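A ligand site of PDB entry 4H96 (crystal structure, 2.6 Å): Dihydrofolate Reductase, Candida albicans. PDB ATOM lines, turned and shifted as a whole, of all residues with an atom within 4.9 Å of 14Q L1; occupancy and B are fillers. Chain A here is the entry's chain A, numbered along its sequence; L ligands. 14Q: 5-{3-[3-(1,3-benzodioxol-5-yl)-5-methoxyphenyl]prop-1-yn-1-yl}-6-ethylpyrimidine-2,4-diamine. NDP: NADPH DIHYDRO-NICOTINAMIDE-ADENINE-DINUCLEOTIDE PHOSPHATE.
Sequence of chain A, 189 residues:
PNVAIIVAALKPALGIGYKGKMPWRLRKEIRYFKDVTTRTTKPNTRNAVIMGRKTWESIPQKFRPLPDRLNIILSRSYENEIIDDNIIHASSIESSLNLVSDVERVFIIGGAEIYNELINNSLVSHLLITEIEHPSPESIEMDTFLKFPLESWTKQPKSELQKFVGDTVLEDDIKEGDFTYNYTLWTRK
NAG of 14Q L1 is in hydrogen-bond range of OE2 of Glu 29, 2.8 Å away. NAI of 14Q L1 sits at hydrogen-bond distance from O of Ile 109, 2.9 Å away. A nitrogen (NAI) of 14Q L1 lies within hydrogen-bond range of the side-chain hydroxyl of Tyr 115 (3.1 Å). A nitrogen (NAI) of 14Q L1 lies within hydrogen-bond range of the backbone carbonyl oxygen of Ile 6. N of Ala 8 sits at hydrogen-bond distance from O7N of NDP L2 (2.8 Å). N7N of NDP L2 is in hydrogen-bond range of O of Ala 8 (3.1 Å). O2D of NDP L2 is in hydrogen-bond range of N of Met 22 (3.3 Å). O2A of NDP L2 lies within hydrogen-bond range of OG1 of Thr 55 (2.5 Å).
OE2 of Glu 29 lies within hydrogen-bond range of OG1 of Thr 130 (3.2 Å). The backbone carbonyl oxygen of Ile 109 lies close to the side-chain hydroxyl of Tyr 115 (3.3 Å). The backbone carbonyl oxygen (O) of Ile 6 lies within hydrogen-bond range of the side-chain hydroxyl (OH) of Tyr 115, at 2.9 Å. The side-chain hydroxyl (OH) of Tyr 115 is in hydrogen-bond range of the backbone NH (N) of Gly 110 (3.3 Å). The backbone NH (N) of Ile 6 is in hydrogen-bond range of the backbone carbonyl oxygen (O) of Ile 108 (3.1 Å). O of Thr 55 is in hydrogen-bond range of OG of Ser 58, 2.7 Å away. The backbone NH (N) of Thr 130 lies within hydrogen-bond range of the backbone carbonyl oxygen (O) of Val 7, 2.8 Å away.
Residues that only touch 14Q L1: Phe 33 (3.5 Å), Ser 58 (3.5 Å), Val 7 (3.6 Å), Ala 8 (3.7 Å), Ile 30 (3.7 Å), Ile 59 (3.7 Å), Met 22 (3.8 Å), Thr 55 (3.9 Å) and Thr 130 (3.9 Å). Hydrophobic or aromatic side chains within 4 Å of 14Q L1: Ile 6, Ala 8, Met 22, Ile 30, Phe 33, Ile 59 and Ile 109. Within 4 Å of 14Q L1: Ile 6, Val 7, Ala 8, Met 22, Glu 29, Ile 30, Phe 33, Thr 55, Ser 58, Ile 59, Ile 109, Tyr 115 and Thr 130. The nearest printed residue that does not touch 14Q L1 is Leu 66 (4.2 Å).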
ATOM      1  N   ILE A   6      18.868  17.708  25.520  1.00  0.00           N
ATOM      2  CA  ILE A   6      19.821  17.223  26.514  1.00  0.00           C
ATOM      3  C   ILE A   6      20.541  15.963  26.009  1.00  0.00           C
ATOM      4  O   ILE A   6      19.897  14.989  25.592  1.00  0.00           O
ATOM      5  CB  ILE A   6      19.141  16.994  27.907  1.00  0.00           C
ATOM      6  CG1 ILE A   6      20.176  16.534  28.953  1.00  0.00           C
ATOM      7  CG2 ILE A   6      17.957  16.028  27.805  1.00  0.00           C
ATOM      8  CD1 ILE A   6      19.730  16.724  30.393  1.00  0.00           C
ATOM      9  N   VAL A   7      21.874  16.010  26.031  1.00  0.00           N
ATOM     10  CA  VAL A   7      22.703  14.931  25.482  1.00  0.00           C
ATOM     11  C   VAL A   7      24.053  14.828  26.190  1.00  0.00           C
ATOM     12  O   VAL A   7      24.587  15.830  26.682  1.00  0.00           O
ATOM     13  CB  VAL A   7      22.890  15.094  23.934  1.00  0.00           C
ATOM     14  CG1 VAL A   7      23.746  16.319  23.587  1.00  0.00           C
ATOM     15  CG2 VAL A   7      23.460  13.835  23.302  1.00  0.00           C
ATOM     16  N   ALA A   8      24.594  13.615  26.259  1.00  0.00           N
ATOM     17  CA  ALA A   8      25.929  13.377  26.786  1.00  0.00           C
ATOM     18  C   ALA A   8      26.846  12.863  25.674  1.00  0.00           C
ATOM     19  O   ALA A   8      26.605  11.797  25.102  1.00  0.00           O
ATOM     20  CB  ALA A   8      25.883  12.383  27.941  1.00  0.00           C
ATOM     21  N   LYS A  21      23.519   0.906  21.827  1.00  0.00           N
ATOM     22  CA  LYS A  21      23.442   1.298  23.248  1.00  0.00           C
ATOM     23  C   LYS A  21      24.621   2.163  23.696  1.00  0.00           C
ATOM     24  O   LYS A  21      25.651   2.238  23.026  1.00  0.00           O
ATOM     25  CB  LYS A  21      23.297   0.054  24.136  1.00  0.00           C
ATOM     26  CG  LYS A  21      21.902  -0.542  24.135  1.00  0.00           C
ATOM     27  CD  LYS A  21      21.816  -1.799  24.983  1.00  0.00           C
ATOM     28  CE  LYS A  21      20.444  -2.440  24.870  1.00  0.00           C
ATOM     29  NZ  LYS A  21      20.373  -3.733  25.611  1.00  0.00           N
ATOM     30  N   MET A  22      24.449   2.816  24.860  1.00  0.00           N
ATOM     31  CA  MET A  22      25.446   3.713  25.422  1.00  0.00           C
ATOM     32  C   MET A  22      26.695   2.957  25.888  1.00  0.00           C
ATOM     33  O   MET A  22      26.582   1.923  26.555  1.00  0.00           O
ATOM     34  CB  MET A  22      24.837   4.500  26.593  1.00  0.00           C
ATOM     35  CG  MET A  22      25.589   5.775  26.964  1.00  0.00           C
ATOM     36  SD  MET A  22      24.764   6.701  28.269  1.00  0.00           S
ATOM     37  CE  MET A  22      23.151   6.954  27.521  1.00  0.00           C
ATOM     38  N   GLU A  29      25.735  11.568  36.388  1.00  0.00           N
ATOM     39  CA  GLU A  29      25.150  12.160  35.183  1.00  0.00           C
ATOM     40  C   GLU A  29      23.679  11.773  35.035  1.00  0.00           C
ATOM     41  O   GLU A  29      22.866  12.575  34.568  1.00  0.00           O
ATOM     42  CB  GLU A  29      25.954  11.742  33.940  1.00  0.00           C
ATOM     43  CG  GLU A  29      25.991  12.783  32.815  1.00  0.00           C
ATOM     44  CD  GLU A  29      24.703  12.854  32.016  1.00  0.00           C
ATOM     45  OE1 GLU A  29      24.129  11.793  31.687  1.00  0.00           O
ATOM     46  OE2 GLU A  29      24.272  13.983  31.689  1.00  0.00           O
ATOM     47  N   ILE A  30      23.352  10.530  35.416  1.00  0.00           N
ATOM     48  CA  ILE A  30      21.967  10.046  35.430  1.00  0.00           C
ATOM     49  C   ILE A  30      21.139  10.810  36.461  1.00  0.00           C
ATOM     50  O   ILE A  30      19.962  11.122  36.225  1.00  0.00           O
ATOM     51  CB  ILE A  30      21.902   8.517  35.673  1.00  0.00           C
ATOM     52  CG1 ILE A  30      22.571   7.754  34.520  1.00  0.00           C
ATOM     53  CG2 ILE A  30      20.453   8.042  35.841  1.00  0.00           C
ATOM     54  CD1 ILE A  30      22.933   6.308  34.842  1.00  0.00           C
ATOM     55  N   PHE A  33      20.421  14.040  34.964  1.00  0.00           N
ATOM     56  CA  PHE A  33      19.408  13.829  33.920  1.00  0.00           C
ATOM     57  C   PHE A  33      17.997  13.766  34.502  1.00  0.00           C
ATOM     58  O   PHE A  33      17.046  14.289  33.919  1.00  0.00           O
ATOM     59  CB  PHE A  33      19.725  12.554  33.135  1.00  0.00           C
ATOM     60  CG  PHE A  33      18.684  12.179  32.115  1.00  0.00           C
ATOM     61  CD1 PHE A  33      18.658  12.808  30.874  1.00  0.00           C
ATOM     62  CD2 PHE A  33      17.743  11.200  32.393  1.00  0.00           C
ATOM     63  CE1 PHE A  33      17.696  12.468  29.919  1.00  0.00           C
ATOM     64  CE2 PHE A  33      16.771  10.849  31.458  1.00  0.00           C
ATOM     65  CZ  PHE A  33      16.753  11.478  30.211  1.00  0.00           C
ATOM     66  N   THR A  55      14.982   4.429  21.097  1.00  0.00           N
ATOM     67  CA  THR A  55      15.371   4.800  22.462  1.00  0.00           C
ATOM     68  C   THR A  55      14.373   4.245  23.475  1.00  0.00           C
ATOM     69  O   THR A  55      14.761   3.742  24.534  1.00  0.00           O
ATOM     70  CB  THR A  55      15.521   6.333  22.623  1.00  0.00           C
ATOM     71  OG1 THR A  55      16.400   6.837  21.608  1.00  0.00           O
ATOM     72  CG2 THR A  55      16.097   6.689  23.991  1.00  0.00           C
ATOM     73  N   SER A  58      15.019   0.598  23.985  1.00  0.00           N
ATOM     74  CA  SER A  58      16.270   0.357  24.705  1.00  0.00           C
ATOM     75  C   SER A  58      16.145   0.642  26.198  1.00  0.00           C
ATOM     76  O   SER A  58      16.849   0.052  27.015  1.00  0.00           O
ATOM     77  CB  SER A  58      17.413   1.171  24.096  1.00  0.00           C
ATOM     78  OG  SER A  58      17.176   2.563  24.225  1.00  0.00           O
ATOM     79  N   ILE A  59      15.248   1.572  26.542  1.00  0.00           N
ATOM     80  CA  ILE A  59      14.930   1.884  27.937  1.00  0.00           C
ATOM     81  C   ILE A  59      14.176   0.709  28.578  1.00  0.00           C
ATOM     82  O   ILE A  59      13.200   0.225  28.002  1.00  0.00           O
ATOM     83  CB  ILE A  59      14.111   3.209  28.047  1.00  0.00           C
ATOM     84  CG1 ILE A  59      14.991   4.415  27.732  1.00  0.00           C
ATOM     85  CG2 ILE A  59      13.481   3.355  29.444  1.00  0.00           C
ATOM     86  CD1 ILE A  59      14.228   5.679  27.353  1.00  0.00           C
ATOM     87  N   PRO A  60      14.656   0.240  29.755  1.00  0.00           N
ATOM     88  CA  PRO A  60      14.059  -0.847  30.528  1.00  0.00           C
ATOM     89  C   PRO A  60      12.535  -0.928  30.420  1.00  0.00           C
ATOM     90  O   PRO A  60      11.846   0.073  30.667  1.00  0.00           O
ATOM     91  CB  PRO A  60      14.483  -0.515  31.954  1.00  0.00           C
ATOM     92  CG  PRO A  60      15.807   0.170  31.795  1.00  0.00           C
ATOM     93  CD  PRO A  60      15.886   0.732  30.397  1.00  0.00           C
ATOM     94  N   LEU A  66       8.889   7.011  31.875  1.00  0.00           N
ATOM     95  CA  LEU A  66       9.621   7.732  32.907  1.00  0.00           C
ATOM     96  C   LEU A  66       8.676   8.479  33.838  1.00  0.00           C
ATOM     97  O   LEU A  66       7.863   9.290  33.371  1.00  0.00           O
ATOM     98  CB  LEU A  66      10.640   8.697  32.283  1.00  0.00           C
ATOM     99  CG  LEU A  66      11.804   8.115  31.463  1.00  0.00           C
ATOM    100  CD1 LEU A  66      12.434   9.187  30.595  1.00  0.00           C
ATOM    101  CD2 LEU A  66      12.854   7.450  32.358  1.00  0.00           C
ATOM    102  N   ILE A 108      14.432  16.917  24.801  1.00  0.00           N
ATOM    103  CA  ILE A 108      14.728  15.919  23.780  1.00  0.00           C
ATOM    104  C   ILE A 108      15.833  14.999  24.314  1.00  0.00           C
ATOM    105  O   ILE A 108      16.962  15.435  24.541  1.00  0.00           O
ATOM    106  CB  ILE A 108      15.166  16.568  22.435  1.00  0.00           C
ATOM    107  CG1 ILE A 108      14.210  17.708  22.023  1.00  0.00           C
ATOM    108  CG2 ILE A 108      15.315  15.510  21.335  1.00  0.00           C
ATOM    109  CD1 ILE A 108      12.737  17.331  21.875  1.00  0.00           C
ATOM    110  N   ILE A 109      15.484  13.730  24.504  1.00  0.00           N
ATOM    111  CA  ILE A 109      16.364  12.785  25.220  1.00  0.00           C
ATOM    112  C   ILE A 109      16.922  11.643  24.362  1.00  0.00           C
ATOM    113  O   ILE A 109      17.498  10.690  24.887  1.00  0.00           O
ATOM    114  CB  ILE A 109      15.678  12.228  26.504  1.00  0.00           C
ATOM    115  CG1 ILE A 109      14.478  11.328  26.144  1.00  0.00           C
ATOM    116  CG2 ILE A 109      15.251  13.369  27.430  1.00  0.00           C
ATOM    117  CD1 ILE A 109      14.114  10.332  27.227  1.00  0.00           C
ATOM    118  N   GLY A 110      16.749  11.740  23.042  1.00  0.00           N
ATOM    119  CA  GLY A 110      17.295  10.739  22.115  1.00  0.00           C
ATOM    120  C   GLY A 110      16.368  10.388  20.965  1.00  0.00           C
ATOM    121  O   GLY A 110      15.179  10.681  21.006  1.00  0.00           O
ATOM    122  N   TYR A 115      18.265  13.649  17.258  1.00  0.00           N
ATOM    123  CA  TYR A 115      19.213  14.721  17.546  1.00  0.00           C
ATOM    124  C   TYR A 115      19.630  15.506  16.297  1.00  0.00           C
ATOM    125  O   TYR A 115      19.629  16.741  16.302  1.00  0.00           O
ATOM    126  CB  TYR A 115      20.459  14.188  18.252  1.00  0.00           C
ATOM    127  CG  TYR A 115      20.278  13.797  19.704  1.00  0.00           C
ATOM    128  CD1 TYR A 115      19.592  14.627  20.599  1.00  0.00           C
ATOM    129  CD2 TYR A 115      20.811  12.611  20.205  1.00  0.00           C
ATOM    130  CE1 TYR A 115      19.436  14.272  21.935  1.00  0.00           C
ATOM    131  CE2 TYR A 115      20.664  12.246  21.535  1.00  0.00           C
ATOM    132  CZ  TYR A 115      19.969  13.086  22.399  1.00  0.00           C
ATOM    133  OH  TYR A 115      19.823  12.733  23.716  1.00  0.00           O
ATOM    134  N   THR A 130      26.412  17.591  27.767  1.00  0.00           N
ATOM    135  CA  THR A 130      27.403  17.190  28.758  1.00  0.00           C
ATOM    136  C   THR A 130      28.673  16.733  28.056  1.00  0.00           C
ATOM    137  O   THR A 130      28.742  15.600  27.549  1.00  0.00           O
ATOM    138  CB  THR A 130      26.863  16.083  29.697  1.00  0.00           C
ATOM    139  OG1 THR A 130      25.555  16.443  30.173  1.00  0.00           O
ATOM    140  CG2 THR A 130      27.789  15.881  30.887  1.00  0.00           C
HETATM  141  CAY 14Q L   1      20.720   9.193  31.470  1.00  0.00           C
HETATM  142  CAH 14Q L   1      21.588   9.203  30.207  1.00  0.00           C
HETATM  143  C4  14Q L   1      21.356  10.484  29.398  1.00  0.00           C
HETATM  144  N3  14Q L   1      22.123  11.599  29.749  1.00  0.00           N
HETATM  145  C2  14Q L   1      21.994  12.825  29.063  1.00  0.00           C
HETATM  146  NAG 14Q L   1      22.726  13.867  29.405  1.00  0.00           N
HETATM  147  N1  14Q L   1      21.067  12.922  28.013  1.00  0.00           N
HETATM  148  C6  14Q L   1      20.300  11.806  27.661  1.00  0.00           C
HETATM  149  NAI 14Q L   1      19.419  11.916  26.662  1.00  0.00           N
HETATM  150  C5  14Q L   1      20.440  10.602  28.350  1.00  0.00           C
HETATM  151  CAJ 14Q L   1      19.629   9.474  27.969  1.00  0.00           C
HETATM  152  CAK 14Q L   1      18.947   8.515  27.640  1.00  0.00           C
HETATM  153  CAL 14Q L   1      18.102   7.385  27.209  1.00  0.00           C
HETATM  154  CAM 14Q L   1      18.343   6.143  28.072  1.00  0.00           C
HETATM  155  CAR 14Q L   1      18.240   6.212  29.459  1.00  0.00           C
HETATM  156  CAN 14Q L   1      18.662   4.934  27.455  1.00  0.00           C
HETATM  157  CAO 14Q L   1      18.877   3.783  28.225  1.00  0.00           C
HETATM  158  OAZ 14Q L   1      19.190   2.603  27.623  1.00  0.00           O
HETATM  159  CBA 14Q L   1      20.603   2.412  27.461  1.00  0.00           C
HETATM  160  CAP 14Q L   1      18.764   3.861  29.617  1.00  0.00           C
HETATM  161  CAQ 14Q L   1      18.460   5.072  30.237  1.00  0.00           C
HETATM  162  CAS 14Q L   1      18.356   5.141  31.623  1.00  0.00           C
HETATM  163  CAX 14Q L   1      17.111   5.302  32.230  1.00  0.00           C
HETATM  164  CAW 14Q L   1      17.007   5.371  33.616  1.00  0.00           C
HETATM  165  OBB 14Q L   1      15.931   5.529  34.446  1.00  0.00           O
HETATM  166  CBC 14Q L   1      16.496   6.019  35.661  1.00  0.00           C
HETATM  167  OBD 14Q L   1      17.782   5.389  35.709  1.00  0.00           O
HETATM  168  CAV 14Q L   1      18.154   5.290  34.404  1.00  0.00           C
HETATM  169  CAU 14Q L   1      19.405   5.129  33.806  1.00  0.00           C
HETATM  170  CAT 14Q L   1      19.503   5.060  32.411  1.00  0.00           C
HETATM  171  PA  NDP L   2      16.330   6.983  17.692  1.00  0.00           P
HETATM  172  O1A NDP L   2      16.762   8.252  17.078  1.00  0.00           O
HETATM  173  O2A NDP L   2      16.010   7.164  19.117  1.00  0.00           O
HETATM  174  O5B NDP L   2      15.047   6.391  16.906  1.00  0.00           O
HETATM  175  C5B NDP L   2      15.061   6.194  15.513  1.00  0.00           C
HETATM  176  C4B NDP L   2      13.688   5.693  15.104  1.00  0.00           C
HETATM  177  O4B NDP L   2      12.705   6.667  15.434  1.00  0.00           O
HETATM  178  C3B NDP L   2      13.588   5.440  13.608  1.00  0.00           C
HETATM  179  O3B NDP L   2      13.757   4.067  13.331  1.00  0.00           O
HETATM  180  C2B NDP L   2      12.189   5.919  13.253  1.00  0.00           C
HETATM  181  O2B NDP L   2      11.291   4.831  13.297  1.00  0.00           O
HETATM  182  C1B NDP L   2      11.823   6.909  14.348  1.00  0.00           C
HETATM  183  N9A NDP L   2      11.992   8.293  13.865  1.00  0.00           N
HETATM  184  C8A NDP L   2      13.175   8.967  13.695  1.00  0.00           C
HETATM  185  N7A NDP L   2      12.916  10.215  13.246  1.00  0.00           N
HETATM  186  C5A NDP L   2      11.588  10.351  13.118  1.00  0.00           C
HETATM  187  C6A NDP L   2      10.790  11.424  12.695  1.00  0.00           C
HETATM  188  N6A NDP L   2      11.346  12.564  12.328  1.00  0.00           N
HETATM  189  N1A NDP L   2       9.415  11.282  12.669  1.00  0.00           N
HETATM  190  C2A NDP L   2       8.832  10.078  13.057  1.00  0.00           C
HETATM  191  N3A NDP L   2       9.630   9.026  13.467  1.00  0.00           N
HETATM  192  C4A NDP L   2      10.990   9.156  13.505  1.00  0.00           C
HETATM  193  O3  NDP L   2      17.461   5.846  17.495  1.00  0.00           O
HETATM  194  PN  NDP L   2      18.969   5.927  16.931  1.00  0.00           P
HETATM  195  O1N NDP L   2      19.472   4.537  16.763  1.00  0.00           O
HETATM  196  O2N NDP L   2      18.989   6.857  15.784  1.00  0.00           O
HETATM  197  O5D NDP L   2      19.763   6.616  18.152  1.00  0.00           O
HETATM  198  C5D NDP L   2      19.910   5.967  19.407  1.00  0.00           C
HETATM  199  C4D NDP L   2      21.383   5.955  19.796  1.00  0.00           C
HETATM  200  O4D NDP L   2      21.728   7.157  20.450  1.00  0.00           O
HETATM  201  C3D NDP L   2      21.688   4.806  20.746  1.00  0.00           C
HETATM  202  O3D NDP L   2      22.706   4.002  20.193  1.00  0.00           O
HETATM  203  C2D NDP L   2      22.142   5.455  22.035  1.00  0.00           C
HETATM  204  O2D NDP L   2      23.337   4.875  22.521  1.00  0.00           O
HETATM  205  C1D NDP L   2      22.365   6.919  21.695  1.00  0.00           C
HETATM  206  N1N NDP L   2      21.834   7.807  22.748  1.00  0.00           N
HETATM  207  C2N NDP L   2      22.709   8.445  23.586  1.00  0.00           C
HETATM  208  C3N NDP L   2      22.247   9.290  24.592  1.00  0.00           C
HETATM  209  C7N NDP L   2      23.206  10.168  25.340  1.00  0.00           C
HETATM  210  O7N NDP L   2      22.829  11.482  25.678  1.00  0.00           O
HETATM  211  N7N NDP L   2      24.405   9.683  25.688  1.00  0.00           N
HETATM  212  C4N NDP L   2      20.875   9.495  24.725  1.00  0.00           C
HETATM  213  C5N NDP L   2      19.989   8.857  23.871  1.00  0.00           C
HETATM  214  C6N NDP L   2      20.484   8.014  22.879  1.00  0.00           C
HETATM  215  P2B NDP L   2       9.950   4.779  12.404  1.00  0.00           P
HETATM  216  O1X NDP L   2       9.179   3.550  12.801  1.00  0.00           O
HETATM  217  O2X NDP L   2       9.103   6.007  12.669  1.00  0.00           O
HETATM  218  O3X NDP L   2      10.305   4.713  10.940  1.00  0.00           O
